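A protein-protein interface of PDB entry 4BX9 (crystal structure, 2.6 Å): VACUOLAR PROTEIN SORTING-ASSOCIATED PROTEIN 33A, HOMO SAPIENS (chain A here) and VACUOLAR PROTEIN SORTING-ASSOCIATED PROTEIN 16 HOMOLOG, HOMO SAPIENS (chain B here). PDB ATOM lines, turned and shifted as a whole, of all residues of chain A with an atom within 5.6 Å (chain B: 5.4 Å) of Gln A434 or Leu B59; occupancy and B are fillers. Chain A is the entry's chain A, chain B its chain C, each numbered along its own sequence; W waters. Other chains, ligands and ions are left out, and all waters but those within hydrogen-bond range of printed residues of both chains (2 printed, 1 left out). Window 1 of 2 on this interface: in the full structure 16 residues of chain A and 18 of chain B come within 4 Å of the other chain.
OG of Ser B58 lies within hydrogen-bond range of O of Thr A435, 3.1 Å away.
N of Leu B59 is in hydrogen-bond range of O of Gln A434 (3.3 Å).
NE2 of Gln A434 sits at hydrogen-bond distance from O of Phe B82, 3.4 Å away.
N of His B60 lies within hydrogen-bond range of O of Gln A434.
OE1 of Gln A434 is in hydrogen-bond range of NH1 of Arg B88, 2.9 Å away.
OD2 of Asp B35 lies within salt-bridge range of NH1 of Arg A430 (3.2 Å).
OE1 of Glu A431 is in salt-bridge range of NE of Arg B88 (3.2 Å).
O of Phe B82 is in hydrogen-bond range of NH2 of Arg A430, 2.9 Å away.
The backbone NH (N) of Asp B61 is in hydrogen-bond range of the side-chain hydroxyl (OG) of Ser B58 (3.0 Å).
The side-chain carboxylate of Asp B61 sits at hydrogen-bond distance from a ring nitrogen (ND1) of His B60, 3.0 Å away.
The side-chain hydroxyl (OG1) of Thr A435 is in hydrogen-bond range of the backbone carbonyl oxygen (O) of Glu A431.
O of Ser B58 sits at hydrogen-bond distance from OG1 of Thr B62, at 2.7 Å.
O of His B60 lies within hydrogen-bond range of OG1 of Thr B64 (2.8 Å).
The side-chain amide nitrogen of Gln A434 lies close to the guanidinium group of Arg A430, 3.3 Å away.
Among the printed residues, merely in contact across the chains: Gln A434 with Ser B58 (3.6 Å), Gly A437 with Ser B58 (3.7 Å), Thr A435 with His B60 (3.8 Å), Gln A434 with Ile B84 (3.9 Å) and Tyr A436 with Ser B58 (3.96 Å).
Gln A434 touches just these residues of chain B: Ser B58, Leu B59, His B60, Phe B82, Ile B84 and Arg B88.
Leu B59 touches just one residue of chain A: Gln A434 (3.3 Å).
Of the printed residues of chain B, Arg A430 touches Asp B35 (3.2 Å) and Phe B82 (2.9 Å).
Printed residues of chain B within 4 Å of Glu A431: Arg B88.
Printed residues of chain B within 4 Å of Gly A437: Ser B58 (3.7 Å).
Of the printed residues of chain A, Ser B58 touches Gln A434 (3.6 Å), Thr A435 (3.1 Å), Tyr A436 (3.96 Å) and Gly A437 (3.7 Å).
Leu A433 touches none of the printed residues of chain B.
The nearest residue of chain A that does not touch Leu B59 is Leu A433 (5.1 Å).
Of the 9 printed residues of chain A, 6 touch a printed residue of chain B.
Water W2 lies within hydrogen-bond range of the guanidinium group (NH1) of Arg B88 (2.7 Å) and the side-chain hydroxyl (OG1) of Thr A435 (2.8 Å).
Water W1 lies within hydrogen-bond range of the backbone carbonyl oxygen of Leu A433, the backbone NH of Leu B59 and the backbone carbonyl oxygen of Gln A434.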
ATOM      1  N   LYS A 429     -12.078 -20.047  -8.949  1.00  0.00           N
ATOM      2  CA  LYS A 429     -12.727 -21.207  -8.321  1.00  0.00           C
ATOM      3  C   LYS A 429     -13.318 -22.199  -9.312  1.00  0.00           C
ATOM      4  O   LYS A 429     -13.140 -23.417  -9.189  1.00  0.00           O
ATOM      5  CB  LYS A 429     -13.780 -20.772  -7.299  1.00  0.00           C
ATOM      6  CG  LYS A 429     -13.140 -20.087  -6.088  1.00  0.00           C
ATOM      7  CD  LYS A 429     -14.031 -20.020  -4.891  1.00  0.00           C
ATOM      8  CE  LYS A 429     -15.171 -19.080  -5.094  1.00  0.00           C
ATOM      9  NZ  LYS A 429     -16.135 -19.356  -4.030  1.00  0.00           N
ATOM     10  N   ARG A 430     -13.997 -21.687 -10.314  1.00  0.00           N
ATOM     11  CA  ARG A 430     -14.574 -22.568 -11.334  1.00  0.00           C
ATOM     12  C   ARG A 430     -13.493 -23.401 -12.023  1.00  0.00           C
ATOM     13  O   ARG A 430     -13.655 -24.594 -12.181  1.00  0.00           O
ATOM     14  CB  ARG A 430     -15.360 -21.737 -12.318  1.00  0.00           C
ATOM     15  CG  ARG A 430     -16.050 -22.470 -13.425  1.00  0.00           C
ATOM     16  CD  ARG A 430     -16.758 -21.427 -14.249  1.00  0.00           C
ATOM     17  NE  ARG A 430     -17.182 -22.047 -15.491  1.00  0.00           N
ATOM     18  CZ  ARG A 430     -18.278 -22.788 -15.616  1.00  0.00           C
ATOM     19  NH1 ARG A 430     -19.085 -22.985 -14.574  1.00  0.00           N
ATOM     20  NH2 ARG A 430     -18.549 -23.350 -16.788  1.00  0.00           N
ATOM     21  N   GLU A 431     -12.364 -22.789 -12.369  1.00  0.00           N
ATOM     22  CA  GLU A 431     -11.322 -23.540 -13.060  1.00  0.00           C
ATOM     23  C   GLU A 431     -10.594 -24.503 -12.132  1.00  0.00           C
ATOM     24  O   GLU A 431     -10.240 -25.603 -12.558  1.00  0.00           O
ATOM     25  CB  GLU A 431     -10.386 -22.692 -13.914  1.00  0.00           C
ATOM     26  CG  GLU A 431      -9.676 -21.523 -13.303  1.00  0.00           C
ATOM     27  CD  GLU A 431      -8.798 -20.910 -14.343  1.00  0.00           C
ATOM     28  OE1 GLU A 431      -9.047 -21.232 -15.527  1.00  0.00           O
ATOM     29  OE2 GLU A 431      -7.874 -20.135 -14.004  1.00  0.00           O
ATOM     30  N   ILE A 432     -10.506 -24.177 -10.842  1.00  0.00           N
ATOM     31  CA  ILE A 432      -9.977 -25.144  -9.860  1.00  0.00           C
ATOM     32  C   ILE A 432     -10.901 -26.333  -9.731  1.00  0.00           C
ATOM     33  O   ILE A 432     -10.442 -27.433  -9.814  1.00  0.00           O
ATOM     34  CB  ILE A 432      -9.681 -24.497  -8.516  1.00  0.00           C
ATOM     35  CG1 ILE A 432      -8.476 -23.563  -8.681  1.00  0.00           C
ATOM     36  CG2 ILE A 432      -9.385 -25.534  -7.406  1.00  0.00           C
ATOM     37  CD1 ILE A 432      -8.248 -22.579  -7.538  1.00  0.00           C
ATOM     38  N   LEU A 433     -12.205 -26.137  -9.561  1.00  0.00           N
ATOM     39  CA  LEU A 433     -13.131 -27.281  -9.490  1.00  0.00           C
ATOM     40  C   LEU A 433     -13.220 -28.123 -10.767  1.00  0.00           C
ATOM     41  O   LEU A 433     -13.338 -29.341 -10.722  1.00  0.00           O
ATOM     42  CB  LEU A 433     -14.554 -26.862  -9.070  1.00  0.00           C
ATOM     43  CG  LEU A 433     -14.684 -26.097  -7.744  1.00  0.00           C
ATOM     44  CD1 LEU A 433     -16.129 -25.652  -7.506  1.00  0.00           C
ATOM     45  CD2 LEU A 433     -14.147 -26.856  -6.536  1.00  0.00           C
ATOM     46  N   GLN A 434     -13.231 -27.470 -11.910  1.00  0.00           N
ATOM     47  CA  GLN A 434     -13.239 -28.229 -13.163  1.00  0.00           C
ATOM     48  C   GLN A 434     -11.985 -29.095 -13.359  1.00  0.00           C
ATOM     49  O   GLN A 434     -12.067 -30.215 -13.879  1.00  0.00           O
ATOM     50  CB  GLN A 434     -13.370 -27.300 -14.346  1.00  0.00           C
ATOM     51  CG  GLN A 434     -14.735 -26.681 -14.451  1.00  0.00           C
ATOM     52  CD  GLN A 434     -14.944 -25.921 -15.738  1.00  0.00           C
ATOM     53  OE1 GLN A 434     -14.012 -25.699 -16.543  1.00  0.00           O
ATOM     54  NE2 GLN A 434     -16.168 -25.520 -15.967  1.00  0.00           N
ATOM     55  N   THR A 435     -10.851 -28.565 -12.958  1.00  0.00           N
ATOM     56  CA  THR A 435      -9.602 -29.237 -13.192  1.00  0.00           C
ATOM     57  C   THR A 435      -9.303 -30.318 -12.127  1.00  0.00           C
ATOM     58  O   THR A 435      -8.810 -31.417 -12.451  1.00  0.00           O
ATOM     59  CB  THR A 435      -8.471 -28.184 -13.192  1.00  0.00           C
ATOM     60  OG1 THR A 435      -8.688 -27.314 -14.286  1.00  0.00           O
ATOM     61  CG2 THR A 435      -7.059 -28.828 -13.297  1.00  0.00           C
ATOM     62  N   TYR A 436      -9.560 -29.995 -10.858  1.00  0.00           N
ATOM     63  CA  TYR A 436      -9.148 -30.861  -9.737  1.00  0.00           C
ATOM     64  C   TYR A 436     -10.308 -31.669  -9.129  1.00  0.00           C
ATOM     65  O   TYR A 436     -10.058 -32.653  -8.456  1.00  0.00           O
ATOM     66  CB  TYR A 436      -8.402 -30.041  -8.678  1.00  0.00           C
ATOM     67  CG  TYR A 436      -7.103 -29.384  -9.202  1.00  0.00           C
ATOM     68  CD1 TYR A 436      -5.907 -30.069  -9.197  1.00  0.00           C
ATOM     69  CD2 TYR A 436      -7.094 -28.061  -9.674  1.00  0.00           C
ATOM     70  CE1 TYR A 436      -4.720 -29.488  -9.668  1.00  0.00           C
ATOM     71  CE2 TYR A 436      -5.923 -27.461 -10.111  1.00  0.00           C
ATOM     72  CZ  TYR A 436      -4.739 -28.178 -10.111  1.00  0.00           C
ATOM     73  OH  TYR A 436      -3.587 -27.600 -10.546  1.00  0.00           O
ATOM     74  N   GLY A 437     -11.563 -31.248  -9.352  1.00  0.00           N
ATOM     75  CA  GLY A 437     -12.734 -31.976  -8.879  1.00  0.00           C
ATOM     76  C   GLY A 437     -13.639 -31.159  -7.991  1.00  0.00           C
ATOM     77  O   GLY A 437     -13.160 -30.363  -7.184  1.00  0.00           O
ATOM     78  N   ASP B  35     -23.605 -27.993 -11.653  1.00  0.00           N
ATOM     79  CA  ASP B  35     -22.656 -28.530 -12.652  1.00  0.00           C
ATOM     80  C   ASP B  35     -22.105 -29.952 -12.358  1.00  0.00           C
ATOM     81  O   ASP B  35     -21.943 -30.777 -13.303  1.00  0.00           O
ATOM     82  CB  ASP B  35     -21.463 -27.553 -12.842  1.00  0.00           C
ATOM     83  CG  ASP B  35     -21.857 -26.342 -13.657  1.00  0.00           C
ATOM     84  OD1 ASP B  35     -22.979 -26.275 -14.165  1.00  0.00           O
ATOM     85  OD2 ASP B  35     -21.074 -25.413 -13.792  1.00  0.00           O
ATOM     86  N   LEU B  39     -22.534 -33.278 -14.520  1.00  0.00           N
ATOM     87  CA  LEU B  39     -21.417 -34.029 -14.982  1.00  0.00           C
ATOM     88  C   LEU B  39     -21.456 -35.473 -14.560  1.00  0.00           C
ATOM     89  O   LEU B  39     -21.087 -36.346 -15.330  1.00  0.00           O
ATOM     90  CB  LEU B  39     -20.160 -33.362 -14.520  1.00  0.00           C
ATOM     91  CG  LEU B  39     -18.903 -34.211 -14.603  1.00  0.00           C
ATOM     92  CD1 LEU B  39     -18.514 -34.233 -16.037  1.00  0.00           C
ATOM     93  CD2 LEU B  39     -17.840 -33.588 -13.748  1.00  0.00           C
ATOM     94  N   GLN B  43     -21.375 -38.610 -16.979  1.00  0.00           N
ATOM     95  CA  GLN B  43     -20.434 -39.665 -16.776  1.00  0.00           C
ATOM     96  C   GLN B  43     -21.086 -41.051 -16.805  1.00  0.00           C
ATOM     97  O   GLN B  43     -20.517 -41.993 -17.300  1.00  0.00           O
ATOM     98  CB  GLN B  43     -19.637 -39.420 -15.495  1.00  0.00           C
ATOM     99  CG  GLN B  43     -18.598 -38.315 -15.633  1.00  0.00           C
ATOM    100  CD  GLN B  43     -17.912 -37.947 -14.329  1.00  0.00           C
ATOM    101  OE1 GLN B  43     -18.367 -38.306 -13.240  1.00  0.00           O
ATOM    102  NE2 GLN B  43     -16.815 -37.226 -14.434  1.00  0.00           N
ATOM    103  N   LEU B  57     -14.555 -38.698 -11.925  1.00  0.00           N
ATOM    104  CA  LEU B  57     -13.495 -37.934 -12.486  1.00  0.00           C
ATOM    105  C   LEU B  57     -13.878 -36.460 -12.507  1.00  0.00           C
ATOM    106  O   LEU B  57     -15.096 -36.086 -12.595  1.00  0.00           O
ATOM    107  CB  LEU B  57     -13.175 -38.407 -13.913  1.00  0.00           C
ATOM    108  CG  LEU B  57     -12.675 -39.852 -14.014  1.00  0.00           C
ATOM    109  CD1 LEU B  57     -12.677 -40.315 -15.470  1.00  0.00           C
ATOM    110  CD2 LEU B  57     -11.294 -39.995 -13.386  1.00  0.00           C
ATOM    111  N   SER B  58     -12.847 -35.634 -12.377  1.00  0.00           N
ATOM    112  CA  SER B  58     -13.013 -34.238 -12.641  1.00  0.00           C
ATOM    113  C   SER B  58     -13.356 -34.034 -14.123  1.00  0.00           C
ATOM    114  O   SER B  58     -13.110 -34.922 -14.988  1.00  0.00           O
ATOM    115  CB  SER B  58     -11.736 -33.473 -12.346  1.00  0.00           C
ATOM    116  OG  SER B  58     -10.697 -33.777 -13.265  1.00  0.00           O
ATOM    117  N   LEU B  59     -13.883 -32.862 -14.429  1.00  0.00           N
ATOM    118  CA  LEU B  59     -14.194 -32.562 -15.817  1.00  0.00           C
ATOM    119  C   LEU B  59     -12.945 -32.679 -16.712  1.00  0.00           C
ATOM    120  O   LEU B  59     -12.990 -33.244 -17.769  1.00  0.00           O
ATOM    121  CB  LEU B  59     -14.830 -31.183 -15.938  1.00  0.00           C
ATOM    122  CG  LEU B  59     -15.021 -30.581 -17.313  1.00  0.00           C
ATOM    123  CD1 LEU B  59     -16.186 -31.262 -17.975  1.00  0.00           C
ATOM    124  CD2 LEU B  59     -15.231 -29.076 -17.174  1.00  0.00           C
ATOM    125  N   HIS B  60     -11.837 -32.167 -16.261  1.00  0.00           N
ATOM    126  CA  HIS B  60     -10.612 -32.205 -17.023  1.00  0.00           C
ATOM    127  C   HIS B  60     -10.166 -33.629 -17.211  1.00  0.00           C
ATOM    128  O   HIS B  60      -9.708 -34.033 -18.276  1.00  0.00           O
ATOM    129  CB  HIS B  60      -9.582 -31.427 -16.237  1.00  0.00           C
ATOM    130  CG  HIS B  60      -8.175 -31.591 -16.709  1.00  0.00           C
ATOM    131  ND1 HIS B  60      -7.385 -32.662 -16.326  1.00  0.00           N
ATOM    132  CD2 HIS B  60      -7.385 -30.784 -17.459  1.00  0.00           C
ATOM    133  CE1 HIS B  60      -6.189 -32.537 -16.879  1.00  0.00           C
ATOM    134  NE2 HIS B  60      -6.151 -31.400 -17.548  1.00  0.00           N
ATOM    135  N   ASP B  61     -10.269 -34.420 -16.167  1.00  0.00           N
ATOM    136  CA  ASP B  61      -9.878 -35.818 -16.301  1.00  0.00           C
ATOM    137  C   ASP B  61     -10.828 -36.615 -17.245  1.00  0.00           C
ATOM    138  O   ASP B  61     -10.405 -37.621 -17.861  1.00  0.00           O
ATOM    139  CB  ASP B  61      -9.759 -36.471 -14.928  1.00  0.00           C
ATOM    140  CG  ASP B  61      -8.516 -36.010 -14.161  1.00  0.00           C
ATOM    141  OD1 ASP B  61      -7.881 -35.005 -14.566  1.00  0.00           O
ATOM    142  OD2 ASP B  61      -8.137 -36.689 -13.187  1.00  0.00           O
ATOM    143  N   THR B  62     -12.070 -36.143 -17.392  1.00  0.00           N
ATOM    144  CA  THR B  62     -13.037 -36.830 -18.216  1.00  0.00           C
ATOM    145  C   THR B  62     -12.750 -36.582 -19.676  1.00  0.00           C
ATOM    146  O   THR B  62     -12.710 -37.500 -20.503  1.00  0.00           O
ATOM    147  CB  THR B  62     -14.465 -36.405 -17.860  1.00  0.00           C
ATOM    148  OG1 THR B  62     -14.677 -36.573 -16.443  1.00  0.00           O
ATOM    149  CG2 THR B  62     -15.463 -37.259 -18.625  1.00  0.00           C
ATOM    150  N   VAL B  63     -12.465 -35.338 -19.976  1.00  0.00           N
ATOM    151  CA  VAL B  63     -12.095 -34.936 -21.322  1.00  0.00           C
ATOM    152  C   VAL B  63     -10.811 -35.680 -21.721  1.00  0.00           C
ATOM    153  O   VAL B  63     -10.752 -36.307 -22.806  1.00  0.00           O
ATOM    154  CB  VAL B  63     -11.943 -33.396 -21.409  1.00  0.00           C
ATOM    155  CG1 VAL B  63     -11.573 -32.936 -22.817  1.00  0.00           C
ATOM    156  CG2 VAL B  63     -13.263 -32.691 -21.026  1.00  0.00           C
ATOM    157  N   THR B  64      -9.818 -35.653 -20.823  1.00  0.00           N
ATOM    158  CA  THR B  64      -8.512 -36.263 -21.062  1.00  0.00           C
ATOM    159  C   THR B  64      -8.721 -37.758 -21.369  1.00  0.00           C
ATOM    160  O   THR B  64      -8.203 -38.291 -22.369  1.00  0.00           O
ATOM    161  CB  THR B  64      -7.514 -36.062 -19.851  1.00  0.00           C
ATOM    162  OG1 THR B  64      -7.260 -34.645 -19.570  1.00  0.00           O
ATOM    163  CG2 THR B  64      -6.168 -36.737 -20.120  1.00  0.00           C
ATOM    164  N   LEU B  78     -17.970 -32.205 -24.857  1.00  0.00           N
ATOM    165  CA  LEU B  78     -18.010 -32.142 -23.422  1.00  0.00           C
ATOM    166  C   LEU B  78     -17.398 -30.814 -22.969  1.00  0.00           C
ATOM    167  O   LEU B  78     -17.961 -30.139 -22.155  1.00  0.00           O
ATOM    168  CB  LEU B  78     -17.339 -33.346 -22.825  1.00  0.00           C
ATOM    169  CG  LEU B  78     -17.243 -33.313 -21.279  1.00  0.00           C
ATOM    170  CD1 LEU B  78     -18.574 -32.991 -20.640  1.00  0.00           C
ATOM    171  CD2 LEU B  78     -16.715 -34.609 -20.642  1.00  0.00           C
ATOM    172  N   PHE B  82     -19.304 -27.290 -20.944  1.00  0.00           N
ATOM    173  CA  PHE B  82     -18.940 -26.566 -19.729  1.00  0.00           C
ATOM    174  C   PHE B  82     -18.117 -25.315 -19.972  1.00  0.00           C
ATOM    175  O   PHE B  82     -17.435 -24.847 -19.068  1.00  0.00           O
ATOM    176  CB  PHE B  82     -18.233 -27.501 -18.714  1.00  0.00           C
ATOM    177  CG  PHE B  82     -19.128 -28.563 -18.153  1.00  0.00           C
ATOM    178  CD1 PHE B  82     -19.374 -29.729 -18.871  1.00  0.00           C
ATOM    179  CD2 PHE B  82     -19.770 -28.372 -16.942  1.00  0.00           C
ATOM    180  CE1 PHE B  82     -20.206 -30.719 -18.380  1.00  0.00           C
ATOM    181  CE2 PHE B  82     -20.618 -29.351 -16.419  1.00  0.00           C
ATOM    182  CZ  PHE B  82     -20.836 -30.532 -17.147  1.00  0.00           C
ATOM    183  N   ILE B  84     -15.337 -24.505 -21.170  1.00  0.00           N
ATOM    184  CA  ILE B  84     -13.874 -24.459 -21.028  1.00  0.00           C
ATOM    185  C   ILE B  84     -13.189 -23.508 -22.056  1.00  0.00           C
ATOM    186  O   ILE B  84     -13.262 -23.714 -23.219  1.00  0.00           O
ATOM    187  CB  ILE B  84     -13.224 -25.847 -21.238  1.00  0.00           C
ATOM    188  CG1 ILE B  84     -13.706 -26.881 -20.212  1.00  0.00           C
ATOM    189  CG2 ILE B  84     -11.739 -25.717 -21.057  1.00  0.00           C
ATOM    190  CD1 ILE B  84     -13.132 -28.269 -20.383  1.00  0.00           C
ATOM    191  N   ARG B  88      -7.214 -23.054 -21.985  1.00  0.00           N
ATOM    192  CA  ARG B  88      -7.197 -24.155 -21.017  1.00  0.00           C
ATOM    193  C   ARG B  88      -7.369 -25.507 -21.736  1.00  0.00           C
ATOM    194  O   ARG B  88      -6.677 -26.461 -21.435  1.00  0.00           O
ATOM    195  CB  ARG B  88      -8.249 -23.929 -19.881  1.00  0.00           C
ATOM    196  CG  ARG B  88      -8.349 -25.050 -18.844  1.00  0.00           C
ATOM    197  CD  ARG B  88      -8.559 -24.523 -17.459  1.00  0.00           C
ATOM    198  NE  ARG B  88      -9.764 -23.753 -17.408  1.00  0.00           N
ATOM    199  CZ  ARG B  88     -10.975 -24.280 -17.200  1.00  0.00           C
ATOM    200  NH1 ARG B  88     -11.198 -25.592 -17.035  1.00  0.00           N
ATOM    201  NH2 ARG B  88     -11.989 -23.463 -17.191  1.00  0.00           N
HETATM  202  O   HOH W   1     -14.846 -31.158 -12.139  1.00  0.00           O
HETATM  203  O   HOH W   2      -9.284 -27.537 -16.976  1.00  0.00           O
